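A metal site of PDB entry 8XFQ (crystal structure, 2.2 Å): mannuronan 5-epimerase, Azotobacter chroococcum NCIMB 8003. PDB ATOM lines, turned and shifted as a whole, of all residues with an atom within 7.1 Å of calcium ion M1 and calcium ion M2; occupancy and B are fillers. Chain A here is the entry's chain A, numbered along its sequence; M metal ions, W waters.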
ATOM      1  N   LEU A 321      -6.050 -16.120 -17.239  1.00  0.00           N
ATOM      2  CA  LEU A 321      -5.972 -17.042 -18.363  1.00  0.00           C
ATOM      3  C   LEU A 321      -7.008 -16.630 -19.403  1.00  0.00           C
ATOM      4  O   LEU A 321      -8.024 -16.008 -19.076  1.00  0.00           O
ATOM      5  CB  LEU A 321      -6.230 -18.487 -17.940  1.00  0.00           C
ATOM      6  CG  LEU A 321      -5.304 -19.202 -16.973  1.00  0.00           C
ATOM      7  CD1 LEU A 321      -5.980 -20.455 -16.441  1.00  0.00           C
ATOM      8  CD2 LEU A 321      -4.004 -19.566 -17.660  1.00  0.00           C
ATOM      9  N   ASN A 322      -6.749 -17.006 -20.649  1.00  0.00           N
ATOM     10  CA  ASN A 322      -7.711 -16.902 -21.735  1.00  0.00           C
ATOM     11  C   ASN A 322      -8.276 -15.491 -21.836  1.00  0.00           C
ATOM     12  O   ASN A 322      -9.489 -15.262 -21.731  1.00  0.00           O
ATOM     13  CB  ASN A 322      -8.816 -17.944 -21.559  1.00  0.00           C
ATOM     14  CG  ASN A 322      -8.301 -19.365 -21.713  1.00  0.00           C
ATOM     15  OD1 ASN A 322      -7.707 -19.719 -22.734  1.00  0.00           O
ATOM     16  ND2 ASN A 322      -8.496 -20.178 -20.676  1.00  0.00           N
ATOM     17  N   SER A 338      -0.769 -12.490 -19.241  1.00  0.00           N
ATOM     18  CA  SER A 338      -1.590 -13.689 -19.192  1.00  0.00           C
ATOM     19  C   SER A 338      -0.667 -14.905 -19.162  1.00  0.00           C
ATOM     20  O   SER A 338       0.558 -14.782 -19.102  1.00  0.00           O
ATOM     21  CB  SER A 338      -2.593 -13.709 -20.354  1.00  0.00           C
ATOM     22  OG  SER A 338      -3.586 -14.697 -20.144  1.00  0.00           O
ATOM     23  N   SER A 339      -1.259 -16.094 -19.253  1.00  0.00           N
ATOM     24  CA  SER A 339      -0.526 -17.337 -19.028  1.00  0.00           C
ATOM     25  C   SER A 339      -1.016 -18.370 -20.045  1.00  0.00           C
ATOM     26  O   SER A 339      -1.592 -18.015 -21.081  1.00  0.00           O
ATOM     27  CB  SER A 339      -0.681 -17.818 -17.575  1.00  0.00           C
ATOM     28  OG  SER A 339       0.072 -19.001 -17.366  1.00  0.00           O
ATOM     29  N   GLU A 340      -0.741 -19.649 -19.758  1.00  0.00           N
ATOM     30  CA  GLU A 340      -1.045 -20.779 -20.631  1.00  0.00           C
ATOM     31  C   GLU A 340      -2.379 -20.636 -21.352  1.00  0.00           C
ATOM     32  O   GLU A 340      -3.382 -20.215 -20.767  1.00  0.00           O
ATOM     33  CB  GLU A 340      -1.042 -22.074 -19.801  1.00  0.00           C
ATOM     34  CG  GLU A 340      -1.309 -23.325 -20.620  1.00  0.00           C
ATOM     35  CD  GLU A 340      -0.198 -23.627 -21.596  1.00  0.00           C
ATOM     36  OE1 GLU A 340       0.849 -24.151 -21.159  1.00  0.00           O
ATOM     37  OE2 GLU A 340      -0.369 -23.328 -22.806  1.00  0.00           O
ATOM     38  N   GLY A 341      -2.383 -20.988 -22.633  1.00  0.00           N
ATOM     39  CA  GLY A 341      -3.525 -20.802 -23.501  1.00  0.00           C
ATOM     40  C   GLY A 341      -3.310 -19.643 -24.463  1.00  0.00           C
ATOM     41  O   GLY A 341      -2.364 -18.864 -24.368  1.00  0.00           O
ATOM     42  N   ARG A 342      -4.242 -19.535 -25.412  1.00  0.00           N
ATOM     43  CA  ARG A 342      -4.146 -18.519 -26.452  1.00  0.00           C
ATOM     44  C   ARG A 342      -4.707 -17.194 -25.930  1.00  0.00           C
ATOM     45  O   ARG A 342      -5.860 -17.140 -25.498  1.00  0.00           O
ATOM     46  CB  ARG A 342      -4.885 -18.962 -27.699  1.00  0.00           C
ATOM     47  CG  ARG A 342      -5.057 -17.875 -28.753  1.00  0.00           C
ATOM     48  CD  ARG A 342      -4.863 -18.445 -30.154  1.00  0.00           C
ATOM     49  NE  ARG A 342      -5.056 -17.441 -31.195  1.00  0.00           N
ATOM     50  CZ  ARG A 342      -4.145 -16.544 -31.547  1.00  0.00           C
ATOM     51  NH1 ARG A 342      -2.949 -16.500 -30.972  1.00  0.00           N
ATOM     52  NH2 ARG A 342      -4.434 -15.677 -32.515  1.00  0.00           N
ATOM     53  N   ASP A 343      -3.891 -16.141 -25.962  1.00  0.00           N
ATOM     54  CA  ASP A 343      -4.305 -14.816 -25.553  1.00  0.00           C
ATOM     55  C   ASP A 343      -4.197 -13.840 -26.713  1.00  0.00           C
ATOM     56  O   ASP A 343      -3.267 -13.936 -27.523  1.00  0.00           O
ATOM     57  CB  ASP A 343      -3.467 -14.319 -24.371  1.00  0.00           C
ATOM     58  CG  ASP A 343      -3.671 -15.143 -23.117  1.00  0.00           C
ATOM     59  OD1 ASP A 343      -4.699 -14.954 -22.434  1.00  0.00           O
ATOM     60  OD2 ASP A 343      -2.789 -15.976 -22.791  1.00  0.00           O
ATOM     61  N   LEU A 344      -5.148 -12.914 -26.793  1.00  0.00           N
ATOM     62  CA  LEU A 344      -5.138 -11.831 -27.770  1.00  0.00           C
ATOM     63  C   LEU A 344      -5.105 -10.521 -26.987  1.00  0.00           C
ATOM     64  O   LEU A 344      -6.112 -10.114 -26.401  1.00  0.00           O
ATOM     65  CB  LEU A 344      -6.372 -11.884 -28.677  1.00  0.00           C
ATOM     66  CG  LEU A 344      -6.759 -13.256 -29.228  1.00  0.00           C
ATOM     67  CD1 LEU A 344      -8.060 -13.171 -30.002  1.00  0.00           C
ATOM     68  CD2 LEU A 344      -5.651 -13.813 -30.088  1.00  0.00           C
ATOM     69  N   LEU A 345      -3.951  -9.865 -26.980  1.00  0.00           N
ATOM     70  CA  LEU A 345      -3.728  -8.696 -26.145  1.00  0.00           C
ATOM     71  C   LEU A 345      -3.326  -7.526 -27.031  1.00  0.00           C
ATOM     72  O   LEU A 345      -2.238  -7.529 -27.628  1.00  0.00           O
ATOM     73  CB  LEU A 345      -2.669  -8.973 -25.075  1.00  0.00           C
ATOM     74  CG  LEU A 345      -2.848 -10.278 -24.288  1.00  0.00           C
ATOM     75  CD1 LEU A 345      -1.599 -10.612 -23.461  1.00  0.00           C
ATOM     76  CD2 LEU A 345      -4.079 -10.216 -23.405  1.00  0.00           C
ATOM     77  N   ASP A 355       2.620  -9.446 -22.311  1.00  0.00           N
ATOM     78  CA  ASP A 355       3.224 -10.751 -22.088  1.00  0.00           C
ATOM     79  C   ASP A 355       2.090 -11.776 -22.045  1.00  0.00           C
ATOM     80  O   ASP A 355       1.325 -11.815 -21.073  1.00  0.00           O
ATOM     81  CB  ASP A 355       4.025 -10.773 -20.797  1.00  0.00           C
ATOM     82  CG  ASP A 355       4.886 -12.031 -20.665  1.00  0.00           C
ATOM     83  OD1 ASP A 355       4.592 -13.037 -21.348  1.00  0.00           O
ATOM     84  OD2 ASP A 355       5.850 -12.007 -19.868  1.00  0.00           O
ATOM     85  N   GLY A 356       1.997 -12.609 -23.074  1.00  0.00           N
ATOM     86  CA  GLY A 356       1.000 -13.651 -23.106  1.00  0.00           C
ATOM     87  C   GLY A 356       1.383 -14.939 -22.401  1.00  0.00           C
ATOM     88  O   GLY A 356       0.565 -15.865 -22.372  1.00  0.00           O
ATOM     89  N   GLY A 357       2.590 -15.033 -21.843  1.00  0.00           N
ATOM     90  CA  GLY A 357       2.985 -16.244 -21.146  1.00  0.00           C
ATOM     91  C   GLY A 357       3.050 -17.443 -22.079  1.00  0.00           C
ATOM     92  O   GLY A 357       3.360 -17.327 -23.269  1.00  0.00           O
ATOM     93  N   ALA A 358       2.739 -18.612 -21.534  1.00  0.00           N
ATOM     94  CA  ALA A 358       2.718 -19.830 -22.334  1.00  0.00           C
ATOM     95  C   ALA A 358       1.609 -19.781 -23.373  1.00  0.00           C
ATOM     96  O   ALA A 358       0.680 -18.967 -23.294  1.00  0.00           O
ATOM     97  CB  ALA A 358       2.551 -21.059 -21.436  1.00  0.00           C
ATOM     98  N   GLY A 359       1.705 -20.665 -24.371  1.00  0.00           N
ATOM     99  CA  GLY A 359       0.708 -20.756 -25.406  1.00  0.00           C
ATOM    100  C   GLY A 359       0.944 -19.774 -26.537  1.00  0.00           C
ATOM    101  O   GLY A 359       1.737 -18.827 -26.441  1.00  0.00           O
ATOM    102  N   ARG A 360       0.228 -19.987 -27.644  1.00  0.00           N
ATOM    103  CA  ARG A 360       0.356 -19.144 -28.824  1.00  0.00           C
ATOM    104  C   ARG A 360      -0.473 -17.882 -28.644  1.00  0.00           C
ATOM    105  O   ARG A 360      -1.704 -17.945 -28.573  1.00  0.00           O
ATOM    106  CB  ARG A 360      -0.065 -19.904 -30.078  1.00  0.00           C
ATOM    107  CG  ARG A 360       0.180 -19.110 -31.362  1.00  0.00           C
ATOM    108  CD  ARG A 360      -0.207 -19.896 -32.605  1.00  0.00           C
ATOM    109  NE  ARG A 360      -1.654 -19.975 -32.770  1.00  0.00           N
ATOM    110  CZ  ARG A 360      -2.386 -19.070 -33.413  1.00  0.00           C
ATOM    111  NH1 ARG A 360      -1.838 -17.991 -33.952  1.00  0.00           N
ATOM    112  NH2 ARG A 360      -3.696 -19.257 -33.513  1.00  0.00           N
ATOM    113  N   ASP A 361       0.185 -16.737 -28.577  1.00  0.00           N
ATOM    114  CA  ASP A 361      -0.477 -15.474 -28.322  1.00  0.00           C
ATOM    115  C   ASP A 361      -0.249 -14.498 -29.473  1.00  0.00           C
ATOM    116  O   ASP A 361       0.786 -14.547 -30.151  1.00  0.00           O
ATOM    117  CB  ASP A 361       0.014 -14.845 -27.013  1.00  0.00           C
ATOM    118  CG  ASP A 361       0.030 -15.833 -25.872  1.00  0.00           C
ATOM    119  OD1 ASP A 361      -1.013 -16.476 -25.626  1.00  0.00           O
ATOM    120  OD2 ASP A 361       1.086 -15.987 -25.230  1.00  0.00           O
ATOM    121  N   THR A 362      -1.223 -13.630 -29.689  1.00  0.00           N
ATOM    122  CA  THR A 362      -1.128 -12.544 -30.647  1.00  0.00           C
ATOM    123  C   THR A 362      -1.137 -11.236 -29.874  1.00  0.00           C
ATOM    124  O   THR A 362      -2.091 -10.943 -29.149  1.00  0.00           O
ATOM    125  CB  THR A 362      -2.276 -12.592 -31.653  1.00  0.00           C
ATOM    126  OG1 THR A 362      -2.208 -13.806 -32.401  1.00  0.00           O
ATOM    127  CG2 THR A 362      -2.207 -11.415 -32.605  1.00  0.00           C
ATOM    128  N   LEU A 363      -0.076 -10.446 -30.038  1.00  0.00           N
ATOM    129  CA  LEU A 363       0.098  -9.213 -29.294  1.00  0.00           C
ATOM    130  C   LEU A 363       0.201  -8.025 -30.241  1.00  0.00           C
ATOM    131  O   LEU A 363       0.730  -8.139 -31.352  1.00  0.00           O
ATOM    132  CB  LEU A 363       1.337  -9.281 -28.396  1.00  0.00           C
ATOM    133  CG  LEU A 363       1.582 -10.621 -27.698  1.00  0.00           C
ATOM    134  CD1 LEU A 363       3.055 -10.819 -27.390  1.00  0.00           C
ATOM    135  CD2 LEU A 363       0.747 -10.737 -26.434  1.00  0.00           C
ATOM    136  N   PHE A 374       8.995 -11.520 -23.226  1.00  0.00           N
ATOM    137  CA  PHE A 374       8.985 -12.977 -23.300  1.00  0.00           C
ATOM    138  C   PHE A 374       9.840 -13.482 -22.151  1.00  0.00           C
ATOM    139  O   PHE A 374      11.074 -13.366 -22.180  1.00  0.00           O
ATOM    140  CB  PHE A 374       9.494 -13.445 -24.666  1.00  0.00           C
ATOM    141  CG  PHE A 374       8.643 -12.985 -25.813  1.00  0.00           C
ATOM    142  CD1 PHE A 374       8.809 -11.717 -26.348  1.00  0.00           C
ATOM    143  CD2 PHE A 374       7.647 -13.803 -26.320  1.00  0.00           C
ATOM    144  CE1 PHE A 374       8.004 -11.282 -27.385  1.00  0.00           C
ATOM    145  CE2 PHE A 374       6.845 -13.377 -27.360  1.00  0.00           C
ATOM    146  CZ  PHE A 374       7.019 -12.104 -27.900  1.00  0.00           C
ATOM    147  N   GLN A 378      10.064 -21.264 -23.416  1.00  0.00           N
ATOM    148  CA  GLN A 378       8.960 -22.118 -23.827  1.00  0.00           C
ATOM    149  C   GLN A 378       7.646 -21.355 -23.981  1.00  0.00           C
ATOM    150  O   GLN A 378       6.604 -21.982 -24.206  1.00  0.00           O
ATOM    151  CB  GLN A 378       8.777 -23.264 -22.836  1.00  0.00           C
ATOM    152  CG  GLN A 378      10.013 -24.146 -22.724  1.00  0.00           C
ATOM    153  CD  GLN A 378      10.321 -24.874 -24.017  1.00  0.00           C
ATOM    154  OE1 GLN A 378      11.429 -24.783 -24.541  1.00  0.00           O
ATOM    155  NE2 GLN A 378       9.334 -25.591 -24.538  1.00  0.00           N
ATOM    156  N   ASP A 379       7.667 -20.026 -23.862  1.00  0.00           N
ATOM    157  CA  ASP A 379       6.459 -19.224 -24.063  1.00  0.00           C
ATOM    158  C   ASP A 379       6.188 -18.942 -25.534  1.00  0.00           C
ATOM    159  O   ASP A 379       5.086 -18.477 -25.851  1.00  0.00           O
ATOM    160  CB  ASP A 379       6.564 -17.901 -23.299  1.00  0.00           C
ATOM    161  CG  ASP A 379       6.533 -18.100 -21.796  1.00  0.00           C
ATOM    162  OD1 ASP A 379       6.088 -19.171 -21.343  1.00  0.00           O
ATOM    163  OD2 ASP A 379       6.946 -17.167 -21.067  1.00  0.00           O
ATOM    164  N   SER A 380       7.152 -19.193 -26.412  1.00  0.00           N
ATOM    165  CA  SER A 380       6.970 -18.968 -27.852  1.00  0.00           C
ATOM    166  C   SER A 380       8.010 -19.830 -28.562  1.00  0.00           C
ATOM    167  O   SER A 380       9.203 -19.504 -28.523  1.00  0.00           O
ATOM    168  CB  SER A 380       7.161 -17.491 -28.193  1.00  0.00           C
ATOM    169  OG  SER A 380       6.773 -17.209 -29.521  1.00  0.00           O
ATOM    170  N   PHE A 381       7.567 -20.913 -29.201  1.00  0.00           N
ATOM    171  CA  PHE A 381       8.523 -21.874 -29.721  1.00  0.00           C
ATOM    172  C   PHE A 381       7.942 -22.682 -30.871  1.00  0.00           C
ATOM    173  O   PHE A 381       6.726 -22.762 -31.060  1.00  0.00           O
ATOM    174  CB  PHE A 381       9.013 -22.829 -28.617  1.00  0.00           C
ATOM    175  CG  PHE A 381       7.944 -23.758 -28.114  1.00  0.00           C
ATOM    176  CD1 PHE A 381       7.041 -23.336 -27.141  1.00  0.00           C
ATOM    177  CD2 PHE A 381       7.843 -25.054 -28.594  1.00  0.00           C
ATOM    178  CE1 PHE A 381       6.060 -24.183 -26.668  1.00  0.00           C
ATOM    179  CE2 PHE A 381       6.858 -25.914 -28.120  1.00  0.00           C
ATOM    180  CZ  PHE A 381       5.965 -25.482 -27.163  1.00  0.00           C
ATOM    181  N   ARG A 390       2.157 -22.504 -31.436  1.00  0.00           N
ATOM    182  CA  ARG A 390       2.867 -22.172 -30.200  1.00  0.00           C
ATOM    183  C   ARG A 390       3.917 -21.084 -30.430  1.00  0.00           C
ATOM    184  O   ARG A 390       4.656 -20.751 -29.484  1.00  0.00           O
ATOM    185  CB  ARG A 390       3.532 -23.380 -29.526  1.00  0.00           C
ATOM    186  CG  ARG A 390       2.912 -23.800 -28.204  1.00  0.00           C
ATOM    187  CD  ARG A 390       1.409 -24.044 -28.325  1.00  0.00           C
ATOM    188  NE  ARG A 390       1.090 -25.212 -29.147  1.00  0.00           N
ATOM    189  CZ  ARG A 390      -0.018 -25.349 -29.861  1.00  0.00           C
ATOM    190  NH1 ARG A 390      -0.933 -24.396 -29.887  1.00  0.00           N
ATOM    191  NH2 ARG A 390      -0.204 -26.457 -30.554  1.00  0.00           N
ATOM    192  N   VAL A 391       4.021 -20.508 -31.625  1.00  0.00           N
ATOM    193  CA  VAL A 391       4.871 -19.350 -31.887  1.00  0.00           C
ATOM    194  C   VAL A 391       4.014 -18.098 -31.797  1.00  0.00           C
ATOM    195  O   VAL A 391       3.003 -17.969 -32.506  1.00  0.00           O
ATOM    196  CB  VAL A 391       5.565 -19.447 -33.251  1.00  0.00           C
ATOM    197  CG1 VAL A 391       6.284 -18.138 -33.563  1.00  0.00           C
ATOM    198  CG2 VAL A 391       6.547 -20.603 -33.283  1.00  0.00           C
ATOM    199  N   ASP A 392       4.415 -17.164 -30.943  1.00  0.00           N
ATOM    200  CA  ASP A 392       3.733 -15.892 -30.815  1.00  0.00           C
ATOM    201  C   ASP A 392       3.940 -15.040 -32.078  1.00  0.00           C
ATOM    202  O   ASP A 392       4.917 -15.207 -32.810  1.00  0.00           O
ATOM    203  CB  ASP A 392       4.258 -15.115 -29.611  1.00  0.00           C
ATOM    204  CG  ASP A 392       3.706 -15.631 -28.298  1.00  0.00           C
ATOM    205  OD1 ASP A 392       3.022 -16.675 -28.298  1.00  0.00           O
ATOM    206  OD2 ASP A 392       3.968 -14.985 -27.260  1.00  0.00           O
HETATM  207 CA    CA M   1       3.184 -17.038 -25.755  1.00  0.00          CA
HETATM  208 CA    CA M   2      -0.894 -17.315 -23.401  1.00  0.00          CA
HETATM  209  O   HOH W   1       4.648 -15.322 -24.724  1.00  0.00           O
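N of Ala 358 lies within hydrogen-bond range of OD1 of Asp 379, 3.4 Å away.
The side-chain carboxylate (OD1) of Asp 343 is in hydrogen-bond range of the side-chain hydroxyl (OG) of Ser 338, at 2.6 Å.
OD1 of Asp 343 is in hydrogen-bond range of N of Asn 322, 3.4 Å away.
The backbone carbonyl oxygen (O) of Asp 343 is in hydrogen-bond range of the backbone NH (N) of Thr 362 (3.0 Å).
The backbone carbonyl oxygen of Ser 338 is in hydrogen-bond range of the backbone NH of Gly 357 (3.4 Å).
N of Gly 357 sits at hydrogen-bond distance from OD1 of Asp 355 (2.9 Å).
The backbone NH of Asp 392 is in hydrogen-bond range of the side-chain hydroxyl of Ser 380 (2.8 Å).
O of Asp 379 is bound to calcium ion M1.
Calcium ion M1 is bound by the backbone carbonyl oxygen (O) of Gly 359.
OD2 of Asp 361 is bound to calcium ion M1 (2.4 Å).
Water W1 binds calcium ion M1, 2.5 Å away.
Calcium ion M1 is bound by the backbone carbonyl oxygen (O) of Gly 357 (2.5 Å).
OD1 of Asp 392 binds calcium ion M1, 2.6 Å away.
OD2 of Asp 392 binds calcium ion M1 (2.7 Å).
Of the 27 residues printed, 6 come within 4 Å of calcium ion M1.
Along chain A the residues within 4 Å of calcium ion M1 span positions 357 to 392.
The nearest printed residue that does not touch calcium ion M1 is Gly 356 (4.3 Å).
Within 4 Å of calcium ion M2: Ser 339, Gly 341, Asp 343, Gly 356, Ala 358 and Asp 361.
The nearest printed residue that does not touch calcium ion M2 is Gly 357 (4.2 Å).
Calcium ion M2 is bound by the backbone carbonyl oxygen (O) of Ala 358.
Calcium ion M2 is bound by O of Gly 356 (2.3 Å).
The backbone carbonyl oxygen (O) of Gly 341 binds calcium ion M2 (2.3 Å).
Calcium ion M2 is bound by the side-chain carboxylate (OD1) of Asp 361.
OD2 of Asp 343 binds calcium ion M2 (2.4 Å).
O of Ser 339 is bound to calcium ion M2, at 2.5 Å.
Slightly farther from calcium ion M2 lies OD2 of Asp 361 (3.0 Å).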
